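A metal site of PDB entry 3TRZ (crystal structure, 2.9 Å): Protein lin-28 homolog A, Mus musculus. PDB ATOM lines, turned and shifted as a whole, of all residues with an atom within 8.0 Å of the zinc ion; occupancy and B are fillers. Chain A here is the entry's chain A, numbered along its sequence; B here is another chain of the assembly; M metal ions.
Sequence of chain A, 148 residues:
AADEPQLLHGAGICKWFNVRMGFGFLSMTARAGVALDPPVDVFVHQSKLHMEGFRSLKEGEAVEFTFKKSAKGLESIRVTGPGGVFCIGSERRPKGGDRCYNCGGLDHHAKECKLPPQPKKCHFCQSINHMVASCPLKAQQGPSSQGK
ND1 of His 130 is in hydrogen-bond range of OG of Ser 127, at 3.4 Å. The side-chain sulfur (SG) of Cys 122 lies close to the backbone NH (N) of Phe 124, 3.4 Å away. The backbone carbonyl oxygen (O) of Ser 127 sits at hydrogen-bond distance from the backbone NH (N) of Cys 122 (2.8 Å). The side-chain sulfur (SG) of Cys 125 sits close to the backbone NH (N) of Ser 127 (3.6 Å). The backbone carbonyl oxygen (O) of Cys 125 sits at hydrogen-bond distance from the backbone NH (N) of Ala 62 (2.8 Å). N of Leu 137 lies close to SG of Cys 135, at 3.5 Å. N of Lys 138 sits close to SG of Cys 135, 3.3 Å away.
NE2 of His 130 is bound to the zinc ion (2.0 Å). SG of Cys 122 binds the zinc ion, 2.2 Å away. The zinc ion is bound by SG of Cys 125, at 2.3 Å. The side-chain sulfur (SG) of Cys 135 is bound to the zinc ion (2.4 Å).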
ATOM      1  N   GLY A  60       8.035  19.070 -26.491  1.00  0.00           N
ATOM      2  CA  GLY A  60       8.277  18.782 -25.085  1.00  0.00           C
ATOM      3  C   GLY A  60       7.337  19.339 -24.034  1.00  0.00           C
ATOM      4  O   GLY A  60       7.457  18.951 -22.863  1.00  0.00           O
ATOM      5  N   GLU A  61       6.402  20.234 -24.431  1.00  0.00           N
ATOM      6  CA  GLU A  61       5.468  20.780 -23.449  1.00  0.00           C
ATOM      7  C   GLU A  61       4.517  19.701 -22.883  1.00  0.00           C
ATOM      8  O   GLU A  61       4.084  18.806 -23.621  1.00  0.00           O
ATOM      9  CB  GLU A  61       4.729  22.041 -23.958  1.00  0.00           C
ATOM     10  CG  GLU A  61       3.638  21.812 -24.992  1.00  0.00           C
ATOM     11  CD  GLU A  61       2.608  22.930 -25.024  1.00  0.00           C
ATOM     12  OE1 GLU A  61       2.602  23.699 -26.014  1.00  0.00           O
ATOM     13  OE2 GLU A  61       1.823  23.034 -24.054  1.00  0.00           O
ATOM     14  N   ALA A  62       4.298  19.732 -21.539  1.00  0.00           N
ATOM     15  CA  ALA A  62       3.474  18.801 -20.770  1.00  0.00           C
ATOM     16  C   ALA A  62       2.099  18.922 -21.256  1.00  0.00           C
ATOM     17  O   ALA A  62       1.585  20.028 -21.479  1.00  0.00           O
ATOM     18  CB  ALA A  62       3.513  19.124 -19.286  1.00  0.00           C
ATOM     19  N   LYS A 121       3.497  24.748 -12.136  1.00  0.00           N
ATOM     20  CA  LYS A 121       3.936  24.108 -13.376  1.00  0.00           C
ATOM     21  C   LYS A 121       5.202  24.801 -13.871  1.00  0.00           C
ATOM     22  O   LYS A 121       5.344  26.004 -13.670  1.00  0.00           O
ATOM     23  CB  LYS A 121       2.815  24.183 -14.433  1.00  0.00           C
ATOM     24  CG  LYS A 121       1.600  23.333 -14.095  1.00  0.00           C
ATOM     25  CD  LYS A 121       0.364  23.756 -14.866  1.00  0.00           C
ATOM     26  CE  LYS A 121      -0.746  24.275 -13.957  1.00  0.00           C
ATOM     27  NZ  LYS A 121      -0.849  25.770 -13.976  1.00  0.00           N
ATOM     28  N   CYS A 122       6.134  24.051 -14.503  1.00  0.00           N
ATOM     29  CA  CYS A 122       7.367  24.600 -15.071  1.00  0.00           C
ATOM     30  C   CYS A 122       7.019  25.783 -15.978  1.00  0.00           C
ATOM     31  O   CYS A 122       6.177  25.663 -16.847  1.00  0.00           O
ATOM     32  CB  CYS A 122       8.139  23.528 -15.834  1.00  0.00           C
ATOM     33  SG  CYS A 122       9.503  24.161 -16.833  1.00  0.00           S
ATOM     34  N   HIS A 123       7.626  26.935 -15.752  1.00  0.00           N
ATOM     35  CA  HIS A 123       7.375  28.128 -16.556  1.00  0.00           C
ATOM     36  C   HIS A 123       7.678  27.955 -18.021  1.00  0.00           C
ATOM     37  O   HIS A 123       7.124  28.687 -18.843  1.00  0.00           O
ATOM     38  CB  HIS A 123       8.142  29.320 -15.994  1.00  0.00           C
ATOM     39  CG  HIS A 123       7.575  29.850 -14.722  1.00  0.00           C
ATOM     40  ND1 HIS A 123       8.393  30.332 -13.710  1.00  0.00           N
ATOM     41  CD2 HIS A 123       6.285  29.995 -14.346  1.00  0.00           C
ATOM     42  CE1 HIS A 123       7.580  30.734 -12.750  1.00  0.00           C
ATOM     43  NE2 HIS A 123       6.304  30.555 -13.088  1.00  0.00           N
ATOM     44  N   PHE A 124       8.521  26.987 -18.360  1.00  0.00           N
ATOM     45  CA  PHE A 124       8.901  26.732 -19.730  1.00  0.00           C
ATOM     46  C   PHE A 124       8.056  25.670 -20.426  1.00  0.00           C
ATOM     47  O   PHE A 124       7.602  25.920 -21.532  1.00  0.00           O
ATOM     48  CB  PHE A 124      10.386  26.363 -19.805  1.00  0.00           C
ATOM     49  CG  PHE A 124      10.931  26.371 -21.218  1.00  0.00           C
ATOM     50  CD1 PHE A 124      10.981  27.547 -21.951  1.00  0.00           C
ATOM     51  CD2 PHE A 124      11.410  25.202 -21.794  1.00  0.00           C
ATOM     52  CE1 PHE A 124      11.501  27.554 -23.251  1.00  0.00           C
ATOM     53  CE2 PHE A 124      11.938  25.216 -23.074  1.00  0.00           C
ATOM     54  CZ  PHE A 124      11.966  26.386 -23.801  1.00  0.00           C
ATOM     55  N   CYS A 125       7.878  24.485 -19.808  1.00  0.00           N
ATOM     56  CA  CYS A 125       7.179  23.353 -20.416  1.00  0.00           C
ATOM     57  C   CYS A 125       5.861  22.953 -19.740  1.00  0.00           C
ATOM     58  O   CYS A 125       5.232  22.004 -20.202  1.00  0.00           O
ATOM     59  CB  CYS A 125       8.127  22.175 -20.497  1.00  0.00           C
ATOM     60  SG  CYS A 125       8.480  21.427 -18.884  1.00  0.00           S
ATOM     61  N   GLN A 126       5.468  23.613 -18.645  1.00  0.00           N
ATOM     62  CA  GLN A 126       4.240  23.320 -17.904  1.00  0.00           C
ATOM     63  C   GLN A 126       4.204  21.968 -17.151  1.00  0.00           C
ATOM     64  O   GLN A 126       3.149  21.602 -16.661  1.00  0.00           O
ATOM     65  CB  GLN A 126       2.996  23.513 -18.754  1.00  0.00           C
ATOM     66  CG  GLN A 126       2.316  24.853 -18.577  1.00  0.00           C
ATOM     67  CD  GLN A 126       1.056  24.963 -19.398  1.00  0.00           C
ATOM     68  OE1 GLN A 126       0.283  25.922 -19.237  1.00  0.00           O
ATOM     69  NE2 GLN A 126       0.808  23.992 -20.317  1.00  0.00           N
ATOM     70  N   SER A 127       5.351  21.275 -17.034  1.00  0.00           N
ATOM     71  CA  SER A 127       5.462  20.026 -16.279  1.00  0.00           C
ATOM     72  C   SER A 127       5.167  20.305 -14.824  1.00  0.00           C
ATOM     73  O   SER A 127       5.591  21.333 -14.280  1.00  0.00           O
ATOM     74  CB  SER A 127       6.863  19.431 -16.395  1.00  0.00           C
ATOM     75  OG  SER A 127       7.125  18.407 -15.446  1.00  0.00           O
ATOM     76  N   ILE A 128       4.454  19.387 -14.176  1.00  0.00           N
ATOM     77  CA  ILE A 128       4.110  19.488 -12.754  1.00  0.00           C
ATOM     78  C   ILE A 128       5.223  18.866 -11.885  1.00  0.00           C
ATOM     79  O   ILE A 128       5.216  19.042 -10.674  1.00  0.00           O
ATOM     80  CB  ILE A 128       2.722  18.873 -12.472  1.00  0.00           C
ATOM     81  CG1 ILE A 128       2.591  17.454 -13.058  1.00  0.00           C
ATOM     82  CG2 ILE A 128       1.584  19.789 -12.945  1.00  0.00           C
ATOM     83  CD1 ILE A 128       2.005  16.463 -12.083  1.00  0.00           C
ATOM     84  N   ASN A 129       6.196  18.178 -12.528  1.00  0.00           N
ATOM     85  CA  ASN A 129       7.289  17.440 -11.902  1.00  0.00           C
ATOM     86  C   ASN A 129       8.540  18.242 -11.573  1.00  0.00           C
ATOM     87  O   ASN A 129       9.353  17.795 -10.741  1.00  0.00           O
ATOM     88  CB  ASN A 129       7.651  16.232 -12.744  1.00  0.00           C
ATOM     89  CG  ASN A 129       6.513  15.250 -12.929  1.00  0.00           C
ATOM     90  OD1 ASN A 129       5.789  14.913 -11.986  1.00  0.00           O
ATOM     91  ND2 ASN A 129       6.320  14.809 -14.160  1.00  0.00           N
ATOM     92  N   HIS A 130       8.746  19.375 -12.253  1.00  0.00           N
ATOM     93  CA  HIS A 130       9.914  20.216 -12.024  1.00  0.00           C
ATOM     94  C   HIS A 130       9.584  21.682 -12.176  1.00  0.00           C
ATOM     95  O   HIS A 130       8.487  22.047 -12.604  1.00  0.00           O
ATOM     96  CB  HIS A 130      11.094  19.829 -12.957  1.00  0.00           C
ATOM     97  CG  HIS A 130      10.824  20.080 -14.404  1.00  0.00           C
ATOM     98  ND1 HIS A 130      10.495  19.064 -15.252  1.00  0.00           N
ATOM     99  CD2 HIS A 130      10.849  21.244 -15.101  1.00  0.00           C
ATOM    100  CE1 HIS A 130      10.314  19.623 -16.442  1.00  0.00           C
ATOM    101  NE2 HIS A 130      10.516  20.938 -16.387  1.00  0.00           N
ATOM    102  N   MET A 131      10.558  22.533 -11.848  1.00  0.00           N
ATOM    103  CA  MET A 131      10.457  23.957 -12.024  1.00  0.00           C
ATOM    104  C   MET A 131      11.545  24.450 -12.954  1.00  0.00           C
ATOM    105  O   MET A 131      12.586  23.813 -13.063  1.00  0.00           O
ATOM    106  CB  MET A 131      10.382  24.685 -10.703  1.00  0.00           C
ATOM    107  CG  MET A 131       9.011  24.551 -10.107  1.00  0.00           C
ATOM    108  SD  MET A 131       8.905  25.355  -8.512  1.00  0.00           S
ATOM    109  CE  MET A 131       7.502  24.490  -7.815  1.00  0.00           C
ATOM    110  N   VAL A 132      11.231  25.505 -13.714  1.00  0.00           N
ATOM    111  CA  VAL A 132      12.073  26.111 -14.767  1.00  0.00           C
ATOM    112  C   VAL A 132      13.583  26.054 -14.530  1.00  0.00           C
ATOM    113  O   VAL A 132      14.308  25.670 -15.441  1.00  0.00           O
ATOM    114  CB  VAL A 132      11.546  27.466 -15.274  1.00  0.00           C
ATOM    115  CG1 VAL A 132      11.808  28.595 -14.305  1.00  0.00           C
ATOM    116  CG2 VAL A 132      12.096  27.780 -16.647  1.00  0.00           C
ATOM    117  N   ALA A 133      14.034  26.334 -13.291  1.00  0.00           N
ATOM    118  CA  ALA A 133      15.447  26.292 -12.918  1.00  0.00           C
ATOM    119  C   ALA A 133      16.093  24.919 -13.078  1.00  0.00           C
ATOM    120  O   ALA A 133      17.324  24.821 -13.088  1.00  0.00           O
ATOM    121  CB  ALA A 133      15.606  26.793 -11.502  1.00  0.00           C
ATOM    122  N   SER A 134      15.271  23.855 -13.202  1.00  0.00           N
ATOM    123  CA  SER A 134      15.735  22.470 -13.376  1.00  0.00           C
ATOM    124  C   SER A 134      15.091  21.812 -14.597  1.00  0.00           C
ATOM    125  O   SER A 134      15.102  20.582 -14.704  1.00  0.00           O
ATOM    126  CB  SER A 134      15.440  21.656 -12.115  1.00  0.00           C
ATOM    127  OG  SER A 134      15.917  22.308 -10.949  1.00  0.00           O
ATOM    128  N   CYS A 135      14.547  22.624 -15.523  1.00  0.00           N
ATOM    129  CA  CYS A 135      13.890  22.158 -16.738  1.00  0.00           C
ATOM    130  C   CYS A 135      14.855  21.482 -17.741  1.00  0.00           C
ATOM    131  O   CYS A 135      15.777  22.140 -18.245  1.00  0.00           O
ATOM    132  CB  CYS A 135      13.106  23.285 -17.401  1.00  0.00           C
ATOM    133  SG  CYS A 135      12.252  22.808 -18.935  1.00  0.00           S
ATOM    134  N   PRO A 136      14.633  20.183 -18.083  1.00  0.00           N
ATOM    135  CA  PRO A 136      15.487  19.509 -19.084  1.00  0.00           C
ATOM    136  C   PRO A 136      15.354  20.135 -20.474  1.00  0.00           C
ATOM    137  O   PRO A 136      16.350  20.266 -21.170  1.00  0.00           O
ATOM    138  CB  PRO A 136      14.967  18.068 -19.100  1.00  0.00           C
ATOM    139  CG  PRO A 136      14.159  17.923 -17.866  1.00  0.00           C
ATOM    140  CD  PRO A 136      13.580  19.272 -17.605  1.00  0.00           C
ATOM    141  N   LEU A 137      14.123  20.499 -20.852  1.00  0.00           N
ATOM    142  CA  LEU A 137      13.785  21.120 -22.133  1.00  0.00           C
ATOM    143  C   LEU A 137      14.535  22.448 -22.297  1.00  0.00           C
ATOM    144  O   LEU A 137      15.129  22.677 -23.351  1.00  0.00           O
ATOM    145  CB  LEU A 137      12.257  21.340 -22.228  1.00  0.00           C
ATOM    146  CG  LEU A 137      11.520  20.943 -23.521  1.00  0.00           C
ATOM    147  CD1 LEU A 137      11.806  21.917 -24.674  1.00  0.00           C
ATOM    148  CD2 LEU A 137      11.795  19.461 -23.900  1.00  0.00           C
ATOM    149  N   LYS A 138      14.517  23.303 -21.266  1.00  0.00           N
ATOM    150  CA  LYS A 138      15.177  24.612 -21.273  1.00  0.00           C
ATOM    151  C   LYS A 138      16.676  24.441 -21.511  1.00  0.00           C
ATOM    152  O   LYS A 138      17.248  25.230 -22.271  1.00  0.00           O
ATOM    153  CB  LYS A 138      14.887  25.372 -19.967  1.00  0.00           C
ATOM    154  CG  LYS A 138      15.360  26.807 -19.950  1.00  0.00           C
ATOM    155  CD  LYS A 138      14.244  27.797 -20.195  1.00  0.00           C
ATOM    156  CE  LYS A 138      14.712  29.191 -19.855  1.00  0.00           C
ATOM    157  NZ  LYS A 138      13.672  30.207 -20.100  1.00  0.00           N
ATOM    158  N   ALA A 139      17.282  23.400 -20.934  1.00  0.00           N
ATOM    159  CA  ALA A 139      18.701  23.070 -21.112  1.00  0.00           C
ATOM    160  C   ALA A 139      18.946  22.456 -22.515  1.00  0.00           C
ATOM    161  O   ALA A 139      19.297  21.280 -22.652  1.00  0.00           O
ATOM    162  CB  ALA A 139      19.152  22.112 -20.024  1.00  0.00           C
ATOM    163  P     G B  18      12.912  30.566  -6.302  1.00  0.00           P
ATOM    164  OP1   G B  18      13.860  30.991  -5.243  1.00  0.00           O
ATOM    165  OP2   G B  18      12.951  29.200  -6.890  1.00  0.00           O
ATOM    166  O5'   G B  18      11.428  30.743  -5.775  1.00  0.00           O
ATOM    167  C5'   G B  18      10.597  31.865  -6.109  1.00  0.00           C
ATOM    168  C4'   G B  18       9.173  31.425  -6.341  1.00  0.00           C
ATOM    169  O4'   G B  18       9.020  31.011  -7.712  1.00  0.00           O
ATOM    170  C3'   G B  18       8.713  30.241  -5.508  1.00  0.00           C
ATOM    171  O3'   G B  18       7.392  30.479  -5.121  1.00  0.00           O
ATOM    172  C2'   G B  18       8.874  29.047  -6.455  1.00  0.00           C
ATOM    173  O2'   G B  18       8.069  27.925  -6.131  1.00  0.00           O
ATOM    174  C1'   G B  18       8.461  29.705  -7.751  1.00  0.00           C
ATOM    175  N9    G B  18       8.918  29.037  -8.966  1.00  0.00           N
ATOM    176  C8    G B  18      10.208  28.876  -9.406  1.00  0.00           C
ATOM    177  N7    G B  18      10.297  28.290 -10.558  1.00  0.00           N
ATOM    178  C5    G B  18       8.964  28.082 -10.939  1.00  0.00           C
ATOM    179  C6    G B  18       8.396  27.468 -12.095  1.00  0.00           C
ATOM    180  O6    G B  18       8.980  26.993 -13.068  1.00  0.00           O
ATOM    181  N1    G B  18       6.987  27.470 -12.089  1.00  0.00           N
ATOM    182  C2    G B  18       6.224  27.994 -11.069  1.00  0.00           C
ATOM    183  N2    G B  18       4.904  27.931 -11.215  1.00  0.00           N
ATOM    184  N3    G B  18       6.737  28.557  -9.983  1.00  0.00           N
ATOM    185  C4    G B  18       8.102  28.563  -9.966  1.00  0.00           C
HETATM  186 ZN    ZN M   1      10.219  22.326 -17.750  1.00  0.00          ZN
